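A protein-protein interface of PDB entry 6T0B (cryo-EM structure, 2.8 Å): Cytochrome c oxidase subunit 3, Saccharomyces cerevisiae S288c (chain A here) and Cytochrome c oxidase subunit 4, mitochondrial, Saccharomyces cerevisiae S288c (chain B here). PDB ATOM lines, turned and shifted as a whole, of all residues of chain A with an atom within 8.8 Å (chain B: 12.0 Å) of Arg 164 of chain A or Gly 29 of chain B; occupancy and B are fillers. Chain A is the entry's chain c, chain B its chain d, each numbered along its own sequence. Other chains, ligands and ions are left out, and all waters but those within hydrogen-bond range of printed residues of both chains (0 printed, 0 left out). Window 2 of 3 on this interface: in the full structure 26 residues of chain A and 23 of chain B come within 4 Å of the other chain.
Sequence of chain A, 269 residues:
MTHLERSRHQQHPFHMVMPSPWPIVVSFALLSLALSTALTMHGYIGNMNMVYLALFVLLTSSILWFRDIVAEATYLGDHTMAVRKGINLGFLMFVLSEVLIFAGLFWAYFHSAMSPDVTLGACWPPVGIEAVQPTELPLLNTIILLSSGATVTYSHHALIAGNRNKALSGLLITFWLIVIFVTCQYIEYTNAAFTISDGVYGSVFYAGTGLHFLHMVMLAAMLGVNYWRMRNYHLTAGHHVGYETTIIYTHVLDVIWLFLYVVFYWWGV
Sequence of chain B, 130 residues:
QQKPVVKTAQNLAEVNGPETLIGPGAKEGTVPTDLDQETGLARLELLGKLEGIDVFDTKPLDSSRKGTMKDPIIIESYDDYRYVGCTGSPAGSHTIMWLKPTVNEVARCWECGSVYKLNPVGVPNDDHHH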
ATOM      1  N   SER A 155      35.388   7.736  -5.536  1.00  0.00           N
ATOM      2  CA  SER A 155      34.319   8.512  -6.149  1.00  0.00           C
ATOM      3  C   SER A 155      33.191   7.609  -6.613  1.00  0.00           C
ATOM      4  O   SER A 155      32.012   7.907  -6.387  1.00  0.00           O
ATOM      5  CB  SER A 155      34.865   9.326  -7.312  1.00  0.00           C
ATOM      6  OG  SER A 155      33.826  10.030  -7.956  1.00  0.00           O
ATOM      7  N   ALA A 158      31.468   6.041  -3.500  1.00  0.00           N
ATOM      8  CA  ALA A 158      30.664   7.025  -2.801  1.00  0.00           C
ATOM      9  C   ALA A 158      29.460   7.441  -3.623  1.00  0.00           C
ATOM     10  O   ALA A 158      28.477   7.928  -3.062  1.00  0.00           O
ATOM     11  CB  ALA A 158      31.510   8.246  -2.456  1.00  0.00           C
ATOM     12  N   LEU A 159      29.529   7.289  -4.945  1.00  0.00           N
ATOM     13  CA  LEU A 159      28.324   7.423  -5.752  1.00  0.00           C
ATOM     14  C   LEU A 159      27.341   6.312  -5.433  1.00  0.00           C
ATOM     15  O   LEU A 159      26.125   6.532  -5.425  1.00  0.00           O
ATOM     16  CB  LEU A 159      28.676   7.420  -7.236  1.00  0.00           C
ATOM     17  CG  LEU A 159      27.532   7.529  -8.239  1.00  0.00           C
ATOM     18  CD1 LEU A 159      26.998   8.925  -8.263  1.00  0.00           C
ATOM     19  CD2 LEU A 159      28.014   7.146  -9.606  1.00  0.00           C
ATOM     20  N   ILE A 160      27.848   5.112  -5.156  1.00  0.00           N
ATOM     21  CA  ILE A 160      26.959   4.035  -4.738  1.00  0.00           C
ATOM     22  C   ILE A 160      26.503   4.234  -3.297  1.00  0.00           C
ATOM     23  O   ILE A 160      25.369   3.899  -2.947  1.00  0.00           O
ATOM     24  CB  ILE A 160      27.654   2.681  -4.943  1.00  0.00           C
ATOM     25  CG1 ILE A 160      28.181   2.583  -6.364  1.00  0.00           C
ATOM     26  CG2 ILE A 160      26.701   1.539  -4.718  1.00  0.00           C
ATOM     27  CD1 ILE A 160      29.009   1.356  -6.613  1.00  0.00           C
ATOM     28  N   ALA A 161      27.341   4.819  -2.451  1.00  0.00           N
ATOM     29  CA  ALA A 161      27.034   4.952  -1.032  1.00  0.00           C
ATOM     30  C   ALA A 161      26.111   6.112  -0.701  1.00  0.00           C
ATOM     31  O   ALA A 161      25.936   6.416   0.479  1.00  0.00           O
ATOM     32  CB  ALA A 161      28.316   5.113  -0.223  1.00  0.00           C
ATOM     33  N   GLY A 162      25.546   6.797  -1.676  1.00  0.00           N
ATOM     34  CA  GLY A 162      24.641   7.870  -1.373  1.00  0.00           C
ATOM     35  C   GLY A 162      25.271   9.236  -1.207  1.00  0.00           C
ATOM     36  O   GLY A 162      24.540  10.231  -1.179  1.00  0.00           O
ATOM     37  N   ASN A 163      26.593   9.324  -1.087  1.00  0.00           N
ATOM     38  CA  ASN A 163      27.248  10.611  -0.903  1.00  0.00           C
ATOM     39  C   ASN A 163      27.263  11.377  -2.209  1.00  0.00           C
ATOM     40  O   ASN A 163      27.474  10.794  -3.273  1.00  0.00           O
ATOM     41  CB  ASN A 163      28.671  10.430  -0.401  1.00  0.00           C
ATOM     42  CG  ASN A 163      28.753  10.408   1.094  1.00  0.00           C
ATOM     43  OD1 ASN A 163      28.686  11.445   1.746  1.00  0.00           O
ATOM     44  ND2 ASN A 163      28.907   9.220   1.657  1.00  0.00           N
ATOM     45  N   ARG A 164      27.021  12.680  -2.138  1.00  0.00           N
ATOM     46  CA  ARG A 164      27.118  13.503  -3.331  1.00  0.00           C
ATOM     47  C   ARG A 164      28.397  14.319  -3.372  1.00  0.00           C
ATOM     48  O   ARG A 164      29.069  14.359  -4.404  1.00  0.00           O
ATOM     49  CB  ARG A 164      25.925  14.442  -3.455  1.00  0.00           C
ATOM     50  CG  ARG A 164      25.892  15.092  -4.803  1.00  0.00           C
ATOM     51  CD  ARG A 164      24.793  16.087  -4.943  1.00  0.00           C
ATOM     52  NE  ARG A 164      24.640  16.494  -6.329  1.00  0.00           N
ATOM     53  CZ  ARG A 164      25.043  17.662  -6.803  1.00  0.00           C
ATOM     54  NH1 ARG A 164      25.611  18.540  -5.999  1.00  0.00           N
ATOM     55  NH2 ARG A 164      24.863  17.954  -8.077  1.00  0.00           N
ATOM     56  N   ASN A 165      28.743  14.974  -2.267  1.00  0.00           N
ATOM     57  CA  ASN A 165      29.936  15.805  -2.255  1.00  0.00           C
ATOM     58  C   ASN A 165      31.197  14.964  -2.290  1.00  0.00           C
ATOM     59  O   ASN A 165      32.196  15.378  -2.880  1.00  0.00           O
ATOM     60  CB  ASN A 165      29.939  16.714  -1.033  1.00  0.00           C
ATOM     61  CG  ASN A 165      28.883  17.802  -1.109  1.00  0.00           C
ATOM     62  OD1 ASN A 165      28.490  18.368  -0.094  1.00  0.00           O
ATOM     63  ND2 ASN A 165      28.421  18.097  -2.314  1.00  0.00           N
ATOM     64  N   LYS A 166      31.171  13.782  -1.691  1.00  0.00           N
ATOM     65  CA  LYS A 166      32.350  12.934  -1.681  1.00  0.00           C
ATOM     66  C   LYS A 166      32.583  12.243  -3.015  1.00  0.00           C
ATOM     67  O   LYS A 166      33.669  11.704  -3.240  1.00  0.00           O
ATOM     68  CB  LYS A 166      32.235  11.895  -0.569  1.00  0.00           C
ATOM     69  CG  LYS A 166      33.558  11.475   0.023  1.00  0.00           C
ATOM     70  CD  LYS A 166      33.367  10.688   1.295  1.00  0.00           C
ATOM     71  CE  LYS A 166      32.811   9.306   1.015  1.00  0.00           C
ATOM     72  NZ  LYS A 166      32.861   8.442   2.225  1.00  0.00           N
ATOM     73  N   ALA A 167      31.590  12.233  -3.896  1.00  0.00           N
ATOM     74  CA  ALA A 167      31.772  11.648  -5.213  1.00  0.00           C
ATOM     75  C   ALA A 167      32.131  12.696  -6.247  1.00  0.00           C
ATOM     76  O   ALA A 167      32.987  12.449  -7.103  1.00  0.00           O
ATOM     77  CB  ALA A 167      30.510  10.906  -5.640  1.00  0.00           C
ATOM     78  N   LEU A 168      31.497  13.868  -6.167  1.00  0.00           N
ATOM     79  CA  LEU A 168      31.819  14.963  -7.074  1.00  0.00           C
ATOM     80  C   LEU A 168      33.240  15.451  -6.864  1.00  0.00           C
ATOM     81  O   LEU A 168      33.953  15.733  -7.831  1.00  0.00           O
ATOM     82  CB  LEU A 168      30.847  16.117  -6.874  1.00  0.00           C
ATOM     83  CG  LEU A 168      29.483  16.000  -7.515  1.00  0.00           C
ATOM     84  CD1 LEU A 168      28.663  17.161  -7.063  1.00  0.00           C
ATOM     85  CD2 LEU A 168      29.630  16.008  -9.002  1.00  0.00           C
ATOM     86  N   SER A 169      33.672  15.536  -5.610  1.00  0.00           N
ATOM     87  CA  SER A 169      35.023  15.992  -5.331  1.00  0.00           C
ATOM     88  C   SER A 169      36.053  14.972  -5.788  1.00  0.00           C
ATOM     89  O   SER A 169      37.104  15.349  -6.313  1.00  0.00           O
ATOM     90  CB  SER A 169      35.177  16.287  -3.848  1.00  0.00           C
ATOM     91  OG  SER A 169      35.056  15.106  -3.092  1.00  0.00           O
ATOM     92  N   GLY A 170      35.765  13.682  -5.618  1.00  0.00           N
ATOM     93  CA  GLY A 170      36.683  12.657  -6.089  1.00  0.00           C
ATOM     94  C   GLY A 170      36.779  12.619  -7.598  1.00  0.00           C
ATOM     95  O   GLY A 170      37.859  12.410  -8.158  1.00  0.00           O
ATOM     96  N   LEU A 171      35.660  12.870  -8.279  1.00  0.00           N
ATOM     97  CA  LEU A 171      35.677  12.973  -9.732  1.00  0.00           C
ATOM     98  C   LEU A 171      36.445  14.199 -10.192  1.00  0.00           C
ATOM     99  O   LEU A 171      37.164  14.148 -11.197  1.00  0.00           O
ATOM    100  CB  LEU A 171      34.251  13.013 -10.254  1.00  0.00           C
ATOM    101  CG  LEU A 171      33.985  12.929 -11.746  1.00  0.00           C
ATOM    102  CD1 LEU A 171      34.909  11.958 -12.408  1.00  0.00           C
ATOM    103  CD2 LEU A 171      32.572  12.467 -11.922  1.00  0.00           C
ATOM    104  N   TYR A 227      31.543  14.345 -14.860  1.00  0.00           N
ATOM    105  CA  TYR A 227      31.331  15.363 -13.834  1.00  0.00           C
ATOM    106  C   TYR A 227      30.105  16.197 -14.139  1.00  0.00           C
ATOM    107  O   TYR A 227      29.355  16.553 -13.224  1.00  0.00           O
ATOM    108  CB  TYR A 227      32.544  16.277 -13.686  1.00  0.00           C
ATOM    109  CG  TYR A 227      32.340  17.352 -12.633  1.00  0.00           C
ATOM    110  CD1 TYR A 227      32.489  17.065 -11.292  1.00  0.00           C
ATOM    111  CD2 TYR A 227      31.987  18.647 -12.981  1.00  0.00           C
ATOM    112  CE1 TYR A 227      32.300  18.030 -10.337  1.00  0.00           C
ATOM    113  CE2 TYR A 227      31.780  19.600 -12.030  1.00  0.00           C
ATOM    114  CZ  TYR A 227      31.941  19.288 -10.714  1.00  0.00           C
ATOM    115  OH  TYR A 227      31.751  20.250  -9.762  1.00  0.00           O
ATOM    116  N   TRP A 228      29.902  16.532 -15.411  1.00  0.00           N
ATOM    117  CA  TRP A 228      28.738  17.317 -15.797  1.00  0.00           C
ATOM    118  C   TRP A 228      27.455  16.569 -15.501  1.00  0.00           C
ATOM    119  O   TRP A 228      26.516  17.123 -14.918  1.00  0.00           O
ATOM    120  CB  TRP A 228      28.799  17.653 -17.274  1.00  0.00           C
ATOM    121  CG  TRP A 228      27.514  18.176 -17.752  1.00  0.00           C
ATOM    122  CD1 TRP A 228      26.861  19.262 -17.278  1.00  0.00           C
ATOM    123  CD2 TRP A 228      26.705  17.646 -18.799  1.00  0.00           C
ATOM    124  NE1 TRP A 228      25.696  19.447 -17.958  1.00  0.00           N
ATOM    125  CE2 TRP A 228      25.579  18.466 -18.901  1.00  0.00           C
ATOM    126  CE3 TRP A 228      26.830  16.563 -19.667  1.00  0.00           C
ATOM    127  CZ2 TRP A 228      24.582  18.239 -19.822  1.00  0.00           C
ATOM    128  CZ3 TRP A 228      25.836  16.336 -20.580  1.00  0.00           C
ATOM    129  CH2 TRP A 228      24.727  17.170 -20.653  1.00  0.00           C
ATOM    130  N   ARG A 229      27.411  15.300 -15.871  1.00  0.00           N
ATOM    131  CA  ARG A 229      26.210  14.517 -15.677  1.00  0.00           C
ATOM    132  C   ARG A 229      25.994  14.120 -14.229  1.00  0.00           C
ATOM    133  O   ARG A 229      24.858  13.840 -13.844  1.00  0.00           O
ATOM    134  CB  ARG A 229      26.263  13.289 -16.571  1.00  0.00           C
ATOM    135  CG  ARG A 229      25.650  13.527 -17.906  1.00  0.00           C
ATOM    136  CD  ARG A 229      26.022  12.462 -18.862  1.00  0.00           C
ATOM    137  NE  ARG A 229      25.871  11.147 -18.276  1.00  0.00           N
ATOM    138  CZ  ARG A 229      24.772  10.420 -18.371  1.00  0.00           C
ATOM    139  NH1 ARG A 229      23.733  10.888 -19.033  1.00  0.00           N
ATOM    140  NH2 ARG A 229      24.718   9.223 -17.817  1.00  0.00           N
ATOM    141  N   MET A 230      27.041  14.104 -13.412  1.00  0.00           N
ATOM    142  CA  MET A 230      26.838  13.860 -11.994  1.00  0.00           C
ATOM    143  C   MET A 230      26.398  15.117 -11.258  1.00  0.00           C
ATOM    144  O   MET A 230      25.598  15.030 -10.322  1.00  0.00           O
ATOM    145  CB  MET A 230      28.115  13.308 -11.373  1.00  0.00           C
ATOM    146  CG  MET A 230      27.927  12.792  -9.983  1.00  0.00           C
ATOM    147  SD  MET A 230      29.477  12.331  -9.216  1.00  0.00           S
ATOM    148  CE  MET A 230      29.815  10.783 -10.030  1.00  0.00           C
ATOM    149  N   ARG A 231      26.896  16.286 -11.660  1.00  0.00           N
ATOM    150  CA  ARG A 231      26.449  17.525 -11.042  1.00  0.00           C
ATOM    151  C   ARG A 231      25.016  17.831 -11.425  1.00  0.00           C
ATOM    152  O   ARG A 231      24.231  18.300 -10.597  1.00  0.00           O
ATOM    153  CB  ARG A 231      27.362  18.672 -11.451  1.00  0.00           C
ATOM    154  CG  ARG A 231      26.984  20.013 -10.883  1.00  0.00           C
ATOM    155  CD  ARG A 231      27.814  21.115 -11.498  1.00  0.00           C
ATOM    156  NE  ARG A 231      27.490  22.428 -10.951  1.00  0.00           N
ATOM    157  CZ  ARG A 231      26.696  23.309 -11.548  1.00  0.00           C
ATOM    158  NH1 ARG A 231      26.146  23.024 -12.713  1.00  0.00           N
ATOM    159  NH2 ARG A 231      26.453  24.479 -10.978  1.00  0.00           N
ATOM    160  N   ASN A 232      24.646  17.551 -12.668  1.00  0.00           N
ATOM    161  CA  ASN A 232      23.298  17.799 -13.137  1.00  0.00           C
ATOM    162  C   ASN A 232      22.378  16.609 -12.936  1.00  0.00           C
ATOM    163  O   ASN A 232      21.352  16.513 -13.616  1.00  0.00           O
ATOM    164  CB  ASN A 232      23.332  18.204 -14.602  1.00  0.00           C
ATOM    165  CG  ASN A 232      23.738  19.630 -14.779  1.00  0.00           C
ATOM    166  OD1 ASN A 232      24.270  20.242 -13.863  1.00  0.00           O
ATOM    167  ND2 ASN A 232      23.484  20.180 -15.954  1.00  0.00           N
ATOM    168  N   TYR A 233      22.739  15.703 -12.028  1.00  0.00           N
ATOM    169  CA  TYR A 233      21.905  14.624 -11.504  1.00  0.00           C
ATOM    170  C   TYR A 233      21.494  13.603 -12.554  1.00  0.00           C
ATOM    171  O   TYR A 233      20.497  12.914 -12.375  1.00  0.00           O
ATOM    172  CB  TYR A 233      20.646  15.154 -10.810  1.00  0.00           C
ATOM    173  CG  TYR A 233      20.865  16.175  -9.726  1.00  0.00           C
ATOM    174  CD1 TYR A 233      20.956  17.513 -10.031  1.00  0.00           C
ATOM    175  CD2 TYR A 233      20.935  15.805  -8.396  1.00  0.00           C
ATOM    176  CE1 TYR A 233      21.139  18.447  -9.073  1.00  0.00           C
ATOM    177  CE2 TYR A 233      21.118  16.748  -7.418  1.00  0.00           C
ATOM    178  CZ  TYR A 233      21.222  18.068  -7.777  1.00  0.00           C
ATOM    179  OH  TYR A 233      21.406  19.048  -6.850  1.00  0.00           O
ATOM    180  N   HIS A 234      22.220  13.478 -13.660  1.00  0.00           N
ATOM    181  CA  HIS A 234      21.910  12.413 -14.605  1.00  0.00           C
ATOM    182  C   HIS A 234      22.330  11.064 -14.050  1.00  0.00           C
ATOM    183  O   HIS A 234      21.563  10.100 -14.096  1.00  0.00           O
ATOM    184  CB  HIS A 234      22.604  12.652 -15.942  1.00  0.00           C
ATOM    185  CG  HIS A 234      22.086  13.825 -16.705  1.00  0.00           C
ATOM    186  ND1 HIS A 234      22.773  15.012 -16.791  1.00  0.00           N
ATOM    187  CD2 HIS A 234      20.966  13.986 -17.441  1.00  0.00           C
ATOM    188  CE1 HIS A 234      22.091  15.861 -17.532  1.00  0.00           C
ATOM    189  NE2 HIS A 234      20.990  15.262 -17.941  1.00  0.00           N
ATOM    190  N   LEU A 235      23.553  10.976 -13.536  1.00  0.00           N
ATOM    191  CA  LEU A 235      24.042   9.747 -12.930  1.00  0.00           C
ATOM    192  C   LEU A 235      23.293   9.447 -11.645  1.00  0.00           C
ATOM    193  O   LEU A 235      23.105  10.321 -10.801  1.00  0.00           O
ATOM    194  CB  LEU A 235      25.523   9.864 -12.618  1.00  0.00           C
ATOM    195  CG  LEU A 235      26.529   9.294 -13.598  1.00  0.00           C
ATOM    196  CD1 LEU A 235      26.586  10.109 -14.834  1.00  0.00           C
ATOM    197  CD2 LEU A 235      27.865   9.293 -12.919  1.00  0.00           C
ATOM    198  N   PRO B  24       9.545  11.085  -9.125  1.00  0.00           N
ATOM    199  CA  PRO B  24       9.874  12.356  -8.487  1.00  0.00           C
ATOM    200  C   PRO B  24      11.370  12.596  -8.565  1.00  0.00           C
ATOM    201  O   PRO B  24      12.172  11.668  -8.591  1.00  0.00           O
ATOM    202  CB  PRO B  24       9.419  12.132  -7.041  1.00  0.00           C
ATOM    203  CG  PRO B  24       9.600  10.672  -6.827  1.00  0.00           C
ATOM    204  CD  PRO B  24       9.374   9.999  -8.147  1.00  0.00           C
ATOM    205  N   GLY B  25      11.755  13.854  -8.615  1.00  0.00           N
ATOM    206  CA  GLY B  25      13.169  14.154  -8.693  1.00  0.00           C
ATOM    207  C   GLY B  25      13.885  13.897  -7.381  1.00  0.00           C
ATOM    208  O   GLY B  25      13.281  13.650  -6.341  1.00  0.00           O
ATOM    209  N   ALA B  26      15.215  13.961  -7.431  1.00  0.00           N
ATOM    210  CA  ALA B  26      15.997  14.036  -6.206  1.00  0.00           C
ATOM    211  C   ALA B  26      15.810  15.414  -5.577  1.00  0.00           C
ATOM    212  O   ALA B  26      15.230  16.310  -6.187  1.00  0.00           O
ATOM    213  CB  ALA B  26      17.467  13.763  -6.493  1.00  0.00           C
ATOM    214  N   LYS B  27      16.305  15.604  -4.350  1.00  0.00           N
ATOM    215  CA  LYS B  27      15.863  16.819  -3.688  1.00  0.00           C
ATOM    216  C   LYS B  27      16.659  18.024  -4.137  1.00  0.00           C
ATOM    217  O   LYS B  27      16.182  18.707  -5.039  1.00  0.00           O
ATOM    218  CB  LYS B  27      15.949  16.664  -2.186  1.00  0.00           C
ATOM    219  CG  LYS B  27      14.974  15.640  -1.633  1.00  0.00           C
ATOM    220  CD  LYS B  27      13.542  16.106  -1.837  1.00  0.00           C
ATOM    221  CE  LYS B  27      12.527  15.024  -1.455  1.00  0.00           C
ATOM    222  NZ  LYS B  27      11.138  15.430  -1.833  1.00  0.00           N
ATOM    223  N   GLU B  28      17.855  18.273  -3.593  1.00  0.00           N
ATOM    224  CA  GLU B  28      18.903  19.005  -4.297  1.00  0.00           C
ATOM    225  C   GLU B  28      20.276  18.472  -3.923  1.00  0.00           C
ATOM    226  O   GLU B  28      21.232  18.609  -4.688  1.00  0.00           O
ATOM    227  CB  GLU B  28      18.886  20.517  -4.027  1.00  0.00           C
ATOM    228  CG  GLU B  28      17.789  21.366  -4.655  1.00  0.00           C
ATOM    229  CD  GLU B  28      17.673  21.208  -6.176  1.00  0.00           C
ATOM    230  OE1 GLU B  28      18.711  21.083  -6.858  1.00  0.00           O
ATOM    231  OE2 GLU B  28      16.527  21.174  -6.696  1.00  0.00           O
ATOM    232  N   GLY B  29      20.398  17.877  -2.748  1.00  0.00           N
ATOM    233  CA  GLY B  29      21.728  17.594  -2.271  1.00  0.00           C
ATOM    234  C   GLY B  29      22.002  16.124  -2.139  1.00  0.00           C
ATOM    235  O   GLY B  29      22.955  15.720  -1.475  1.00  0.00           O
ATOM    236  N   THR B  30      21.168  15.318  -2.776  1.00  0.00           N
ATOM    237  CA  THR B  30      21.241  13.873  -2.695  1.00  0.00           C
ATOM    238  C   THR B  30      21.523  13.317  -4.073  1.00  0.00           C
ATOM    239  O   THR B  30      21.016  13.834  -5.068  1.00  0.00           O
ATOM    240  CB  THR B  30      19.937  13.286  -2.184  1.00  0.00           C
ATOM    241  OG1 THR B  30      18.874  13.689  -3.051  1.00  0.00           O
ATOM    242  CG2 THR B  30      19.644  13.774  -0.791  1.00  0.00           C
ATOM    243  N   VAL B  31      22.334  12.275  -4.138  1.00  0.00           N
ATOM    244  CA  VAL B  31      22.444  11.558  -5.410  1.00  0.00           C
ATOM    245  C   VAL B  31      21.148  10.792  -5.648  1.00  0.00           C
ATOM    246  O   VAL B  31      20.543  10.297  -4.682  1.00  0.00           O
ATOM    247  CB  VAL B  31      23.675  10.640  -5.404  1.00  0.00           C
ATOM    248  CG1 VAL B  31      23.628   9.679  -4.307  1.00  0.00           C
ATOM    249  CG2 VAL B  31      23.815   9.892  -6.690  1.00  0.00           C
ATOM    250  N   PRO B  32      20.602  10.795  -6.860  1.00  0.00           N
ATOM    251  CA  PRO B  32      19.330  10.110  -7.086  1.00  0.00           C
ATOM    252  C   PRO B  32      19.495   8.608  -6.991  1.00  0.00           C
ATOM    253  O   PRO B  32      20.465   8.047  -7.492  1.00  0.00           O
ATOM    254  CB  PRO B  32      18.949  10.538  -8.503  1.00  0.00           C
ATOM    255  CG  PRO B  32      19.675  11.780  -8.720  1.00  0.00           C
ATOM    256  CD  PRO B  32      20.947  11.660  -7.996  1.00  0.00           C
ATOM    257  N   THR B  33      18.570   7.967  -6.304  1.00  0.00           N
ATOM    258  CA  THR B  33      18.432   6.539  -6.481  1.00  0.00           C
ATOM    259  C   THR B  33      17.373   6.300  -7.538  1.00  0.00           C
ATOM    260  O   THR B  33      16.625   7.200  -7.912  1.00  0.00           O
ATOM    261  CB  THR B  33      18.080   5.840  -5.177  1.00  0.00           C
ATOM    262  OG1 THR B  33      18.130   4.427  -5.386  1.00  0.00           O
ATOM    263  CG2 THR B  33      16.703   6.224  -4.724  1.00  0.00           C
ATOM    264  N   ASP B  36      13.780   7.324  -7.847  1.00  0.00           N
ATOM    265  CA  ASP B  36      13.503   8.720  -8.145  1.00  0.00           C
ATOM    266  C   ASP B  36      13.497   8.980  -9.646  1.00  0.00           C
ATOM    267  O   ASP B  36      12.483   9.389 -10.214  1.00  0.00           O
ATOM    268  CB  ASP B  36      14.524   9.622  -7.456  1.00  0.00           C
ATOM    269  CG  ASP B  36      14.321   9.699  -5.968  1.00  0.00           C
ATOM    270  OD1 ASP B  36      13.327  10.312  -5.535  1.00  0.00           O
ATOM    271  OD2 ASP B  36      15.152   9.142  -5.226  1.00  0.00           O
ATOM    272  N   GLN B  37      14.612   8.722 -10.314  1.00  0.00           N
ATOM    273  CA  GLN B  37      14.756   9.231 -11.667  1.00  0.00           C
ATOM    274  C   GLN B  37      14.973   8.165 -12.728  1.00  0.00           C
ATOM    275  O   GLN B  37      15.876   8.296 -13.558  1.00  0.00           O
ATOM    276  CB  GLN B  37      15.913  10.212 -11.720  1.00  0.00           C
ATOM    277  CG  GLN B  37      15.710  11.422 -10.878  1.00  0.00           C
ATOM    278  CD  GLN B  37      16.930  12.258 -10.854  1.00  0.00           C
ATOM    279  OE1 GLN B  37      17.870  11.994 -11.589  1.00  0.00           O
ATOM    280  NE2 GLN B  37      16.934  13.287 -10.026  1.00  0.00           N
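Of the 24 printed residues of chain A, 5 touch a printed residue of chain B. Of the 12 printed residues of chain B, 6 touch a printed residue of chain A. Printed residues of chain B that touch a printed residue of chain A: Glu 28, Gly 29, Thr 30, Val 31, Pro 32 and Gln 37. Hydrophobic or aromatic side chains of chain B that line the printed part of chain A: Val 31 and Pro 32. Among the printed residues, 8 pairs touch across the chains.
NH2 of Arg 164 of chain A is in hydrogen-bond range of O of Arg 231 of chain A (2.6 Å). The backbone NH (N) of Leu 235 of chain A is in hydrogen-bond range of the backbone carbonyl oxygen (O) of Arg 229 of chain A, 3.2 Å away. The side-chain amide nitrogen of Gln 37 of chain B lies close to the backbone NH of Ala 26 of chain B (3.2 Å). The side-chain hydroxyl (OG1) of Thr 30 of chain B lies within hydrogen-bond range of the backbone NH (N) of Lys 27 of chain B, at 3.5 Å.
Arg 164 of chain A touches just one residue of chain B: Gly 29 (3.8 Å). Gly 29 of chain B touches just one residue of chain A: Arg 164. Ala 161 of chain A touches none of the printed residues of chain B. Gly 162 of chain A touches just one residue of chain B: Val 31 (3.3 Å). No residue of chain B comes within 4 Å of Asn 163 of chain A. No residue of chain B comes within 4 Å of Asn 165 of chain A. No residue of chain B comes within 4 Å of Ala 167 of chain A. No residue of chain B comes within 4 Å of Arg 231 of chain A. Of chain A, only Tyr 233 (3.7 Å) comes within 4 Å of Thr 30 of chain B. Of the printed residues of chain A, Val 31 of chain B touches Leu 159 and Gly 162. Printed residues of chain A within 4 Å of Pro 32 of chain B: Tyr 233 and Leu 235. Of the printed residues of chain A, Gln 37 of chain B touches Tyr 233 (2.9 Å). The nearest residue of chain B that does not touch Arg 164 of chain A is Val 31 of chain B (4.2 Å). The nearest printed residue of chain A that does not touch Val 31 of chain B is Asn 163 of chain A (4.1 Å).
Among the printed residues, pairs that only touch across the chains: Gly 162 of chain A with Val 31 of chain B, Leu 159 of chain A with Val 31 of chain B, Tyr 233 of chain A with Thr 30 of chain B, Leu 235 of chain A with Pro 32 of chain B, Arg 164 of chain A with Gly 29 of chain B and Tyr 233 of chain A with Pro 32 of chain B.
OE1 of Glu 28 of chain B sits close to OH of Tyr 233 of chain A. The backbone carbonyl oxygen (O) of Tyr 233 of chain A lies close to the side-chain amide oxygen (OE1) of Gln 37 of chain B, 2.9 Å away.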
